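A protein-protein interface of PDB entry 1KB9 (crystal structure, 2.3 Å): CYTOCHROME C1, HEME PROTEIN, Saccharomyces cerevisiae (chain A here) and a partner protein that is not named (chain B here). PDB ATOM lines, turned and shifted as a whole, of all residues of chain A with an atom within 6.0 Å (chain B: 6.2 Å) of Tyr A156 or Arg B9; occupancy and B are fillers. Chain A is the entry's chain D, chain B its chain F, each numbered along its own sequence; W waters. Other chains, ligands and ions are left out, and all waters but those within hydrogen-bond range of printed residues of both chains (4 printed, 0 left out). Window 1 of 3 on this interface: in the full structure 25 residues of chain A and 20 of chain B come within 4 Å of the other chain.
O of Thr A135 sits at hydrogen-bond distance from NH2 of Arg B9 (3.1 Å).
The side-chain hydroxyl (OH) of Tyr A156 sits at hydrogen-bond distance from the side-chain carboxylate (OD2) of Asp B62 (2.6 Å).
The backbone carbonyl oxygen (O) of Pro A155 lies within hydrogen-bond range of the backbone NH (N) of Leu A8, 2.8 Å away.
The side-chain amide oxygen (OD1) of Asn A154 lies within hydrogen-bond range of the backbone NH (N) of Tyr A156 (3.2 Å).
The guanidinium group (NH1) of Arg B9 lies close to the side-chain amide nitrogen (NE2) of Gln B58 (3.4 Å).
NH1 of Arg B9 is in salt-bridge range of OD1 of Asp B62, 3.7 Å away.
Among the printed residues, merely in contact across the chains: Leu A8 with Gln B58, Thr A135 with Leu B5, Tyr A156 with Gln B58, Pro A155 with Phe B55, Leu A8 with Phe B55, Tyr A156 with Arg B9, Pro A11 with Asp B62 and Leu A8 with Asp B62.
Of the printed residues of chain B, Tyr A156 touches Arg B9, Gln B58 and Asp B62.
Of the printed residues of chain A, Leu B5 touches Thr A135.
Printed residues of chain B within 4 Å of Leu A8: Phe B55 (3.8 Å), Gln B58 (3.4 Å) and Asp B62 (3.8 Å).
Of the printed residues of chain B, Thr A135 touches Leu B5 (3.6 Å) and Arg B9 (3.1 Å).
Printed residues of chain A within 4 Å of Asp B62: Leu A8 (3.8 Å), Pro A11 (3.8 Å) and Tyr A156 (2.6 Å).
The nearest residue of chain B that does not touch Tyr A156 is Phe B55 (5.8 Å).
Of the 18 printed residues of chain A, 5 touch a printed residue of chain B.
Printed residues of chain A that touch a printed residue of chain B: Leu A8, Pro A11, Thr A135, Pro A155 and Tyr A156.
Hydrophobic or aromatic side chains of chain A that line the printed part of chain B: Leu A8, Pro A11, Pro A155 and Tyr A156.
Along chain A the printed residues that touch a printed residue of chain B span positions 8 to 156.
Of the 16 printed residues of chain B, 5 touch a printed residue of chain A.
Printed residues of chain B that touch a printed residue of chain A: Leu B5, Arg B9, Phe B55, Gln B58 and Asp B62.
Hydrophobic or aromatic side chains of chain B that line the printed part of chain A: Leu B5 and Phe B55.
Water W3 bridges O of His A9 (2.7 Å) and OD2 of Asp B62 (2.8 Å).
Water W2 lies within hydrogen-bond range of O of Ser A132 (2.7 Å), OG1 of Thr A135 (2.8 Å), NH1 of Arg B9 (3.1 Å) and N of Gly A136 (3.2 Å).
Water W4 lies within hydrogen-bond range of the side-chain hydroxyl (OH) of Tyr A13, the side-chain hydroxyl (OH) of Tyr A156, the side-chain hydroxyl (OG) of Ser A132, the side-chain carboxylate (OD1) of Asp B62 and the guanidinium group (NH1) of Arg B9.
Water W1 lies within hydrogen-bond range of O of Gly A136 (2.8 Å) and NE2 of Gln B58 (3.1 Å).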
ATOM      1  N   HIS A   6      42.422 -22.574  24.975  1.00  0.00           N
ATOM      2  CA  HIS A   6      42.078 -23.024  26.325  1.00  0.00           C
ATOM      3  C   HIS A   6      40.827 -23.877  26.311  1.00  0.00           C
ATOM      4  O   HIS A   6      40.745 -24.874  27.022  1.00  0.00           O
ATOM      5  CB  HIS A   6      41.819 -21.838  27.268  1.00  0.00           C
ATOM      6  CG  HIS A   6      43.055 -21.261  27.888  1.00  0.00           C
ATOM      7  ND1 HIS A   6      43.981 -22.029  28.564  1.00  0.00           N
ATOM      8  CD2 HIS A   6      43.505 -19.984  27.955  1.00  0.00           C
ATOM      9  CE1 HIS A   6      44.948 -21.250  29.019  1.00  0.00           C
ATOM     10  NE2 HIS A   6      44.683 -20.006  28.663  1.00  0.00           N
ATOM     11  N   GLY A   7      39.859 -23.464  25.497  1.00  0.00           N
ATOM     12  CA  GLY A   7      38.588 -24.156  25.411  1.00  0.00           C
ATOM     13  C   GLY A   7      37.597 -23.421  26.294  1.00  0.00           C
ATOM     14  O   GLY A   7      37.991 -22.778  27.273  1.00  0.00           O
ATOM     15  N   LEU A   8      36.315 -23.497  25.952  1.00  0.00           N
ATOM     16  CA  LEU A   8      35.278 -22.821  26.725  1.00  0.00           C
ATOM     17  C   LEU A   8      35.112 -23.464  28.094  1.00  0.00           C
ATOM     18  O   LEU A   8      35.059 -24.685  28.218  1.00  0.00           O
ATOM     19  CB  LEU A   8      33.941 -22.877  25.987  1.00  0.00           C
ATOM     20  CG  LEU A   8      33.024 -21.651  25.981  1.00  0.00           C
ATOM     21  CD1 LEU A   8      31.635 -22.110  25.624  1.00  0.00           C
ATOM     22  CD2 LEU A   8      33.002 -20.943  27.308  1.00  0.00           C
ATOM     23  N   HIS A   9      35.031 -22.627  29.118  1.00  0.00           N
ATOM     24  CA  HIS A   9      34.844 -23.095  30.481  1.00  0.00           C
ATOM     25  C   HIS A   9      33.458 -23.730  30.595  1.00  0.00           C
ATOM     26  O   HIS A   9      32.455 -23.122  30.223  1.00  0.00           O
ATOM     27  CB  HIS A   9      34.963 -21.911  31.453  1.00  0.00           C
ATOM     28  CG  HIS A   9      34.554 -22.233  32.860  1.00  0.00           C
ATOM     29  ND1 HIS A   9      33.381 -21.767  33.419  1.00  0.00           N
ATOM     30  CD2 HIS A   9      35.158 -22.978  33.819  1.00  0.00           C
ATOM     31  CE1 HIS A   9      33.280 -22.212  34.661  1.00  0.00           C
ATOM     32  NE2 HIS A   9      34.345 -22.949  34.927  1.00  0.00           N
ATOM     33  N   ALA A  10      33.411 -24.960  31.088  1.00  0.00           N
ATOM     34  CA  ALA A  10      32.152 -25.663  31.260  1.00  0.00           C
ATOM     35  C   ALA A  10      31.441 -25.113  32.492  1.00  0.00           C
ATOM     36  O   ALA A  10      32.065 -24.902  33.530  1.00  0.00           O
ATOM     37  CB  ALA A  10      32.395 -27.155  31.405  1.00  0.00           C
ATOM     38  N   PRO A  11      30.132 -24.827  32.375  1.00  0.00           N
ATOM     39  CA  PRO A  11      29.319 -24.294  33.470  1.00  0.00           C
ATOM     40  C   PRO A  11      28.953 -25.382  34.474  1.00  0.00           C
ATOM     41  O   PRO A  11      29.066 -26.576  34.177  1.00  0.00           O
ATOM     42  CB  PRO A  11      28.087 -23.778  32.738  1.00  0.00           C
ATOM     43  CG  PRO A  11      27.916 -24.789  31.665  1.00  0.00           C
ATOM     44  CD  PRO A  11      29.324 -24.969  31.150  1.00  0.00           C
ATOM     45  N   TYR A  13      26.348 -27.557  36.262  1.00  0.00           N
ATOM     46  CA  TYR A  13      24.995 -28.113  36.269  1.00  0.00           C
ATOM     47  C   TYR A  13      24.670 -28.678  37.649  1.00  0.00           C
ATOM     48  O   TYR A  13      25.575 -29.060  38.396  1.00  0.00           O
ATOM     49  CB  TYR A  13      24.856 -29.192  35.199  1.00  0.00           C
ATOM     50  CG  TYR A  13      24.860 -28.613  33.811  1.00  0.00           C
ATOM     51  CD1 TYR A  13      23.763 -27.892  33.340  1.00  0.00           C
ATOM     52  CD2 TYR A  13      25.974 -28.737  32.982  1.00  0.00           C
ATOM     53  CE1 TYR A  13      23.774 -27.300  32.080  1.00  0.00           C
ATOM     54  CE2 TYR A  13      25.996 -28.147  31.716  1.00  0.00           C
ATOM     55  CZ  TYR A  13      24.892 -27.427  31.273  1.00  0.00           C
ATOM     56  OH  TYR A  13      24.906 -26.814  30.038  1.00  0.00           O
ATOM     57  N   TYR A 129      32.101 -31.081  32.306  1.00  0.00           N
ATOM     58  CA  TYR A 129      32.820 -31.078  31.040  1.00  0.00           C
ATOM     59  C   TYR A 129      32.245 -32.087  30.054  1.00  0.00           C
ATOM     60  O   TYR A 129      31.885 -31.722  28.949  1.00  0.00           O
ATOM     61  CB  TYR A 129      34.320 -31.339  31.254  1.00  0.00           C
ATOM     62  CG  TYR A 129      35.070 -31.584  29.969  1.00  0.00           C
ATOM     63  CD1 TYR A 129      35.286 -30.549  29.057  1.00  0.00           C
ATOM     64  CD2 TYR A 129      35.512 -32.857  29.632  1.00  0.00           C
ATOM     65  CE1 TYR A 129      35.917 -30.779  27.838  1.00  0.00           C
ATOM     66  CE2 TYR A 129      36.147 -33.099  28.416  1.00  0.00           C
ATOM     67  CZ  TYR A 129      36.343 -32.053  27.525  1.00  0.00           C
ATOM     68  OH  TYR A 129      36.954 -32.285  26.314  1.00  0.00           O
ATOM     69  N   SER A 132      28.745 -31.041  28.855  1.00  0.00           N
ATOM     70  CA  SER A 132      28.861 -29.881  27.986  1.00  0.00           C
ATOM     71  C   SER A 132      29.431 -30.222  26.620  1.00  0.00           C
ATOM     72  O   SER A 132      28.980 -29.695  25.610  1.00  0.00           O
ATOM     73  CB  SER A 132      29.693 -28.791  28.656  1.00  0.00           C
ATOM     74  OG  SER A 132      29.012 -28.258  29.782  1.00  0.00           O
ATOM     75  N   LEU A 133      30.410 -31.116  26.585  1.00  0.00           N
ATOM     76  CA  LEU A 133      31.016 -31.514  25.323  1.00  0.00           C
ATOM     77  C   LEU A 133      29.979 -32.197  24.427  1.00  0.00           C
ATOM     78  O   LEU A 133      29.831 -31.837  23.260  1.00  0.00           O
ATOM     79  CB  LEU A 133      32.188 -32.475  25.563  1.00  0.00           C
ATOM     80  CG  LEU A 133      32.914 -32.966  24.302  1.00  0.00           C
ATOM     81  CD1 LEU A 133      33.881 -31.902  23.810  1.00  0.00           C
ATOM     82  CD2 LEU A 133      33.652 -34.262  24.578  1.00  0.00           C
ATOM     83  N   THR A 135      26.714 -32.063  24.460  1.00  0.00           N
ATOM     84  CA  THR A 135      25.597 -31.214  24.083  1.00  0.00           C
ATOM     85  C   THR A 135      26.046 -29.864  23.521  1.00  0.00           C
ATOM     86  O   THR A 135      25.220 -28.982  23.272  1.00  0.00           O
ATOM     87  CB  THR A 135      24.708 -30.944  25.302  1.00  0.00           C
ATOM     88  OG1 THR A 135      25.493 -30.333  26.332  1.00  0.00           O
ATOM     89  CG2 THR A 135      24.109 -32.237  25.829  1.00  0.00           C
ATOM     90  N   GLY A 136      27.346 -29.713  23.297  1.00  0.00           N
ATOM     91  CA  GLY A 136      27.860 -28.446  22.815  1.00  0.00           C
ATOM     92  C   GLY A 136      28.324 -28.346  21.383  1.00  0.00           C
ATOM     93  O   GLY A 136      29.130 -27.476  21.080  1.00  0.00           O
ATOM     94  N   TYR A 137      27.866 -29.239  20.510  1.00  0.00           N
ATOM     95  CA  TYR A 137      28.244 -29.176  19.095  1.00  0.00           C
ATOM     96  C   TYR A 137      27.332 -28.180  18.370  1.00  0.00           C
ATOM     97  O   TYR A 137      26.112 -28.346  18.360  1.00  0.00           O
ATOM     98  CB  TYR A 137      28.103 -30.546  18.423  1.00  0.00           C
ATOM     99  CG  TYR A 137      29.192 -31.538  18.756  1.00  0.00           C
ATOM    100  CD1 TYR A 137      29.056 -32.423  19.826  1.00  0.00           C
ATOM    101  CD2 TYR A 137      30.343 -31.627  17.972  1.00  0.00           C
ATOM    102  CE1 TYR A 137      30.031 -33.370  20.102  1.00  0.00           C
ATOM    103  CE2 TYR A 137      31.325 -32.571  18.241  1.00  0.00           C
ATOM    104  CZ  TYR A 137      31.162 -33.439  19.307  1.00  0.00           C
ATOM    105  OH  TYR A 137      32.127 -34.376  19.575  1.00  0.00           O
ATOM    106  N   ASN A 154      33.742 -27.943  18.432  1.00  0.00           N
ATOM    107  CA  ASN A 154      33.116 -28.018  19.740  1.00  0.00           C
ATOM    108  C   ASN A 154      33.886 -26.986  20.547  1.00  0.00           C
ATOM    109  O   ASN A 154      35.108 -27.086  20.687  1.00  0.00           O
ATOM    110  CB  ASN A 154      33.291 -29.408  20.341  1.00  0.00           C
ATOM    111  CG  ASN A 154      32.356 -29.655  21.499  1.00  0.00           C
ATOM    112  OD1 ASN A 154      32.335 -28.893  22.470  1.00  0.00           O
ATOM    113  ND2 ASN A 154      31.561 -30.715  21.402  1.00  0.00           N
ATOM    114  N   PRO A 155      33.190 -25.968  21.074  1.00  0.00           N
ATOM    115  CA  PRO A 155      33.840 -24.914  21.859  1.00  0.00           C
ATOM    116  C   PRO A 155      34.452 -25.363  23.188  1.00  0.00           C
ATOM    117  O   PRO A 155      35.407 -24.756  23.667  1.00  0.00           O
ATOM    118  CB  PRO A 155      32.709 -23.910  22.065  1.00  0.00           C
ATOM    119  CG  PRO A 155      31.517 -24.799  22.200  1.00  0.00           C
ATOM    120  CD  PRO A 155      31.726 -25.802  21.089  1.00  0.00           C
ATOM    121  N   TYR A 156      33.923 -26.436  23.770  1.00  0.00           N
ATOM    122  CA  TYR A 156      34.420 -26.934  25.053  1.00  0.00           C
ATOM    123  C   TYR A 156      35.717 -27.737  24.984  1.00  0.00           C
ATOM    124  O   TYR A 156      36.392 -27.908  25.993  1.00  0.00           O
ATOM    125  CB  TYR A 156      33.327 -27.728  25.760  1.00  0.00           C
ATOM    126  CG  TYR A 156      32.086 -26.905  25.992  1.00  0.00           C
ATOM    127  CD1 TYR A 156      30.979 -27.023  25.148  1.00  0.00           C
ATOM    128  CD2 TYR A 156      32.023 -25.983  27.036  1.00  0.00           C
ATOM    129  CE1 TYR A 156      29.840 -26.238  25.337  1.00  0.00           C
ATOM    130  CE2 TYR A 156      30.892 -25.194  27.235  1.00  0.00           C
ATOM    131  CZ  TYR A 156      29.802 -25.331  26.377  1.00  0.00           C
ATOM    132  OH  TYR A 156      28.684 -24.563  26.564  1.00  0.00           O
ATOM    133  N   PHE A 157      36.067 -28.212  23.795  1.00  0.00           N
ATOM    134  CA  PHE A 157      37.287 -28.982  23.597  1.00  0.00           C
ATOM    135  C   PHE A 157      38.426 -27.998  23.300  1.00  0.00           C
ATOM    136  O   PHE A 157      38.247 -27.050  22.532  1.00  0.00           O
ATOM    137  CB  PHE A 157      37.098 -29.938  22.419  1.00  0.00           C
ATOM    138  CG  PHE A 157      38.205 -30.941  22.255  1.00  0.00           C
ATOM    139  CD1 PHE A 157      38.381 -31.966  23.185  1.00  0.00           C
ATOM    140  CD2 PHE A 157      39.066 -30.871  21.161  1.00  0.00           C
ATOM    141  CE1 PHE A 157      39.401 -32.912  23.024  1.00  0.00           C
ATOM    142  CE2 PHE A 157      40.086 -31.803  20.991  1.00  0.00           C
ATOM    143  CZ  PHE A 157      40.257 -32.829  21.924  1.00  0.00           C
ATOM    144  N   PRO A 158      39.596 -28.180  23.944  1.00  0.00           N
ATOM    145  CA  PRO A 158      40.758 -27.304  23.741  1.00  0.00           C
ATOM    146  C   PRO A 158      41.161 -27.279  22.280  1.00  0.00           C
ATOM    147  O   PRO A 158      41.402 -28.325  21.683  1.00  0.00           O
ATOM    148  CB  PRO A 158      41.835 -27.968  24.600  1.00  0.00           C
ATOM    149  CG  PRO A 158      41.038 -28.545  25.734  1.00  0.00           C
ATOM    150  CD  PRO A 158      39.869 -29.172  25.003  1.00  0.00           C
ATOM    151  N   GLN B   4      15.328 -30.131  25.925  1.00  0.00           N
ATOM    152  CA  GLN B   4      15.228 -29.156  27.004  1.00  0.00           C
ATOM    153  C   GLN B   4      16.307 -28.077  26.995  1.00  0.00           C
ATOM    154  O   GLN B   4      16.046 -26.928  27.360  1.00  0.00           O
ATOM    155  CB  GLN B   4      15.221 -29.874  28.354  1.00  0.00           C
ATOM    156  CG  GLN B   4      14.053 -30.839  28.567  1.00  0.00           C
ATOM    157  CD  GLN B   4      14.327 -32.259  28.084  1.00  0.00           C
ATOM    158  OE1 GLN B   4      13.707 -33.211  28.560  1.00  0.00           O
ATOM    159  NE2 GLN B   4      15.254 -32.408  27.145  1.00  0.00           N
ATOM    160  N   LEU B   5      17.520 -28.449  26.596  1.00  0.00           N
ATOM    161  CA  LEU B   5      18.628 -27.505  26.542  1.00  0.00           C
ATOM    162  C   LEU B   5      18.441 -26.531  25.374  1.00  0.00           C
ATOM    163  O   LEU B   5      18.581 -25.317  25.545  1.00  0.00           O
ATOM    164  CB  LEU B   5      19.959 -28.255  26.424  1.00  0.00           C
ATOM    165  CG  LEU B   5      21.263 -27.454  26.471  1.00  0.00           C
ATOM    166  CD1 LEU B   5      21.336 -26.609  27.728  1.00  0.00           C
ATOM    167  CD2 LEU B   5      22.433 -28.406  26.413  1.00  0.00           C
ATOM    168  N   GLU B   6      18.108 -27.064  24.198  1.00  0.00           N
ATOM    169  CA  GLU B   6      17.882 -26.239  23.010  1.00  0.00           C
ATOM    170  C   GLU B   6      16.777 -25.226  23.262  1.00  0.00           C
ATOM    171  O   GLU B   6      16.814 -24.112  22.741  1.00  0.00           O
ATOM    172  CB  GLU B   6      17.496 -27.103  21.810  1.00  0.00           C
ATOM    173  CG  GLU B   6      18.662 -27.767  21.121  1.00  0.00           C
ATOM    174  CD  GLU B   6      18.601 -27.602  19.615  1.00  0.00           C
ATOM    175  OE1 GLU B   6      18.116 -28.532  18.931  1.00  0.00           O
ATOM    176  OE2 GLU B   6      19.032 -26.534  19.117  1.00  0.00           O
ATOM    177  N   ASP B   7      15.795 -25.635  24.060  1.00  0.00           N
ATOM    178  CA  ASP B   7      14.665 -24.791  24.416  1.00  0.00           C
ATOM    179  C   ASP B   7      15.148 -23.594  25.234  1.00  0.00           C
ATOM    180  O   ASP B   7      14.910 -22.448  24.859  1.00  0.00           O
ATOM    181  CB  ASP B   7      13.648 -25.604  25.223  1.00  0.00           C
ATOM    182  CG  ASP B   7      12.390 -24.819  25.546  1.00  0.00           C
ATOM    183  OD1 ASP B   7      11.407 -24.941  24.782  1.00  0.00           O
ATOM    184  OD2 ASP B   7      12.381 -24.094  26.569  1.00  0.00           O
ATOM    185  N   LEU B   8      15.839 -23.872  26.341  1.00  0.00           N
ATOM    186  CA  LEU B   8      16.368 -22.827  27.218  1.00  0.00           C
ATOM    187  C   LEU B   8      17.376 -21.915  26.521  1.00  0.00           C
ATOM    188  O   LEU B   8      17.474 -20.730  26.842  1.00  0.00           O
ATOM    189  CB  LEU B   8      16.985 -23.438  28.479  1.00  0.00           C
ATOM    190  CG  LEU B   8      16.013 -23.914  29.559  1.00  0.00           C
ATOM    191  CD1 LEU B   8      16.777 -24.561  30.699  1.00  0.00           C
ATOM    192  CD2 LEU B   8      15.210 -22.736  30.071  1.00  0.00           C
ATOM    193  N   ARG B   9      18.134 -22.463  25.576  1.00  0.00           N
ATOM    194  CA  ARG B   9      19.101 -21.657  24.843  1.00  0.00           C
ATOM    195  C   ARG B   9      18.365 -20.678  23.938  1.00  0.00           C
ATOM    196  O   ARG B   9      18.576 -19.468  24.026  1.00  0.00           O
ATOM    197  CB  ARG B   9      20.057 -22.543  24.038  1.00  0.00           C
ATOM    198  CG  ARG B   9      21.189 -23.097  24.887  1.00  0.00           C
ATOM    199  CD  ARG B   9      22.146 -23.999  24.124  1.00  0.00           C
ATOM    200  NE  ARG B   9      23.295 -24.322  24.967  1.00  0.00           N
ATOM    201  CZ  ARG B   9      24.148 -25.320  24.754  1.00  0.00           C
ATOM    202  NH1 ARG B   9      25.156 -25.503  25.597  1.00  0.00           N
ATOM    203  NH2 ARG B   9      24.000 -26.134  23.715  1.00  0.00           N
ATOM    204  N   GLU B  10      17.451 -21.203  23.125  1.00  0.00           N
ATOM    205  CA  GLU B  10      16.653 -20.392  22.209  1.00  0.00           C
ATOM    206  C   GLU B  10      15.956 -19.284  22.996  1.00  0.00           C
ATOM    207  O   GLU B  10      15.985 -18.115  22.606  1.00  0.00           O
ATOM    208  CB  GLU B  10      15.618 -21.268  21.495  1.00  0.00           C
ATOM    209  CG  GLU B  10      15.037 -20.653  20.229  1.00  0.00           C
ATOM    210  CD  GLU B  10      16.107 -20.329  19.194  1.00  0.00           C
ATOM    211  OE1 GLU B  10      16.984 -21.188  18.943  1.00  0.00           O
ATOM    212  OE2 GLU B  10      16.073 -19.208  18.634  1.00  0.00           O
ATOM    213  N   HIS B  11      15.382 -19.653  24.136  1.00  0.00           N
ATOM    214  CA  HIS B  11      14.698 -18.700  24.994  1.00  0.00           C
ATOM    215  C   HIS B  11      15.610 -17.547  25.419  1.00  0.00           C
ATOM    216  O   HIS B  11      15.202 -16.387  25.361  1.00  0.00           O
ATOM    217  CB  HIS B  11      14.145 -19.405  26.233  1.00  0.00           C
ATOM    218  CG  HIS B  11      13.623 -18.469  27.276  1.00  0.00           C
ATOM    219  ND1 HIS B  11      12.382 -17.875  27.190  1.00  0.00           N
ATOM    220  CD2 HIS B  11      14.185 -18.002  28.416  1.00  0.00           C
ATOM    221  CE1 HIS B  11      12.202 -17.082  28.232  1.00  0.00           C
ATOM    222  NE2 HIS B  11      13.281 -17.140  28.992  1.00  0.00           N
ATOM    223  N   PHE B  12      16.840 -17.864  25.831  1.00  0.00           N
ATOM    224  CA  PHE B  12      17.787 -16.840  26.277  1.00  0.00           C
ATOM    225  C   PHE B  12      18.466 -16.035  25.175  1.00  0.00           C
ATOM    226  O   PHE B  12      18.875 -14.893  25.400  1.00  0.00           O
ATOM    227  CB  PHE B  12      18.800 -17.415  27.275  1.00  0.00           C
ATOM    228  CG  PHE B  12      18.245 -17.556  28.666  1.00  0.00           C
ATOM    229  CD1 PHE B  12      17.813 -18.789  29.140  1.00  0.00           C
ATOM    230  CD2 PHE B  12      18.095 -16.439  29.483  1.00  0.00           C
ATOM    231  CE1 PHE B  12      17.234 -18.908  30.405  1.00  0.00           C
ATOM    232  CE2 PHE B  12      17.516 -16.545  30.750  1.00  0.00           C
ATOM    233  CZ  PHE B  12      17.085 -17.781  31.208  1.00  0.00           C
ATOM    234  N   LYS B  13      18.559 -16.612  23.980  1.00  0.00           N
ATOM    235  CA  LYS B  13      19.145 -15.902  22.847  1.00  0.00           C
ATOM    236  C   LYS B  13      18.215 -14.735  22.476  1.00  0.00           C
ATOM    237  O   LYS B  13      18.621 -13.799  21.785  1.00  0.00           O
ATOM    238  CB  LYS B  13      19.304 -16.841  21.647  1.00  0.00           C
ATOM    239  CG  LYS B  13      20.192 -18.046  21.913  1.00  0.00           C
ATOM    240  CD  LYS B  13      20.167 -19.072  20.773  1.00  0.00           C
ATOM    241  CE  LYS B  13      21.144 -18.729  19.656  1.00  0.00           C
ATOM    242  NZ  LYS B  13      20.834 -17.437  18.981  1.00  0.00           N
ATOM    243  N   ASN B  14      16.975 -14.790  22.967  1.00  0.00           N
ATOM    244  CA  ASN B  14      15.982 -13.756  22.684  1.00  0.00           C
ATOM    245  C   ASN B  14      15.682 -12.774  23.810  1.00  0.00           C
ATOM    246  O   ASN B  14      14.634 -12.127  23.812  1.00  0.00           O
ATOM    247  CB  ASN B  14      14.685 -14.377  22.151  1.00  0.00           C
ATOM    248  CG  ASN B  14      14.810 -14.827  20.705  1.00  0.00           C
ATOM    249  OD1 ASN B  14      14.968 -14.004  19.798  1.00  0.00           O
ATOM    250  ND2 ASN B  14      14.761 -16.137  20.485  1.00  0.00           N
ATOM    251  N   PHE B  55      32.234 -17.109  21.934  1.00  0.00           N
ATOM    252  CA  PHE B  55      32.424 -17.530  23.322  1.00  0.00           C
ATOM    253  C   PHE B  55      31.619 -16.664  24.289  1.00  0.00           C
ATOM    254  O   PHE B  55      31.060 -17.179  25.257  1.00  0.00           O
ATOM    255  CB  PHE B  55      33.913 -17.519  23.708  1.00  0.00           C
ATOM    256  CG  PHE B  55      34.644 -18.806  23.398  1.00  0.00           C
ATOM    257  CD1 PHE B  55      35.742 -19.193  24.163  1.00  0.00           C
ATOM    258  CD2 PHE B  55      34.252 -19.618  22.341  1.00  0.00           C
ATOM    259  CE1 PHE B  55      36.447 -20.372  23.879  1.00  0.00           C
ATOM    260  CE2 PHE B  55      34.947 -20.800  22.046  1.00  0.00           C
ATOM    261  CZ  PHE B  55      36.049 -21.176  22.820  1.00  0.00           C
ATOM    262  N   GLN B  58      28.015 -17.903  23.951  1.00  0.00           N
ATOM    263  CA  GLN B  58      27.918 -19.203  24.600  1.00  0.00           C
ATOM    264  C   GLN B  58      28.077 -19.118  26.116  1.00  0.00           C
ATOM    265  O   GLN B  58      27.373 -19.814  26.854  1.00  0.00           O
ATOM    266  CB  GLN B  58      28.950 -20.160  24.024  1.00  0.00           C
ATOM    267  CG  GLN B  58      28.595 -21.608  24.247  1.00  0.00           C
ATOM    268  CD  GLN B  58      27.405 -22.063  23.418  1.00  0.00           C
ATOM    269  OE1 GLN B  58      26.987 -21.386  22.462  1.00  0.00           O
ATOM    270  NE2 GLN B  58      26.863 -23.228  23.767  1.00  0.00           N
ATOM    271  N   LEU B  61      24.840 -17.822  27.611  1.00  0.00           N
ATOM    272  CA  LEU B  61      23.845 -18.884  27.549  1.00  0.00           C
ATOM    273  C   LEU B  61      24.095 -19.952  28.617  1.00  0.00           C
ATOM    274  O   LEU B  61      23.157 -20.419  29.270  1.00  0.00           O
ATOM    275  CB  LEU B  61      23.824 -19.506  26.149  1.00  0.00           C
ATOM    276  CG  LEU B  61      23.458 -18.549  25.006  1.00  0.00           C
ATOM    277  CD1 LEU B  61      23.543 -19.284  23.665  1.00  0.00           C
ATOM    278  CD2 LEU B  61      22.057 -17.963  25.229  1.00  0.00           C
ATOM    279  N   ASP B  62      25.364 -20.320  28.800  1.00  0.00           N
ATOM    280  CA  ASP B  62      25.747 -21.317  29.797  1.00  0.00           C
ATOM    281  C   ASP B  62      25.368 -20.839  31.197  1.00  0.00           C
ATOM    282  O   ASP B  62      24.774 -21.580  31.980  1.00  0.00           O
ATOM    283  CB  ASP B  62      27.257 -21.585  29.744  1.00  0.00           C
ATOM    284  CG  ASP B  62      27.654 -22.519  28.616  1.00  0.00           C
ATOM    285  OD1 ASP B  62      26.793 -23.274  28.123  1.00  0.00           O
ATOM    286  OD2 ASP B  62      28.843 -22.512  28.227  1.00  0.00           O
ATOM    287  N   THR B  65      21.446 -21.082  31.388  1.00  0.00           N
ATOM    288  CA  THR B  65      20.862 -22.411  31.239  1.00  0.00           C
ATOM    289  C   THR B  65      21.316 -23.456  32.262  1.00  0.00           C
ATOM    290  O   THR B  65      20.517 -24.281  32.707  1.00  0.00           O
ATOM    291  CB  THR B  65      21.101 -22.971  29.821  1.00  0.00           C
ATOM    292  OG1 THR B  65      22.506 -23.121  29.591  1.00  0.00           O
ATOM    293  CG2 THR B  65      20.524 -22.035  28.775  1.00  0.00           C
HETATM  294  O   HOH W   1      28.127 -24.922  21.562  1.00  0.00           O
HETATM  295  O   HOH W   2      26.948 -28.002  25.956  1.00  0.00           O
HETATM  296  O   HOH W   3      30.465 -21.354  30.221  1.00  0.00           O
HETATM  297  O   HOH W   4      27.016 -26.387  28.332  1.00  0.00           O
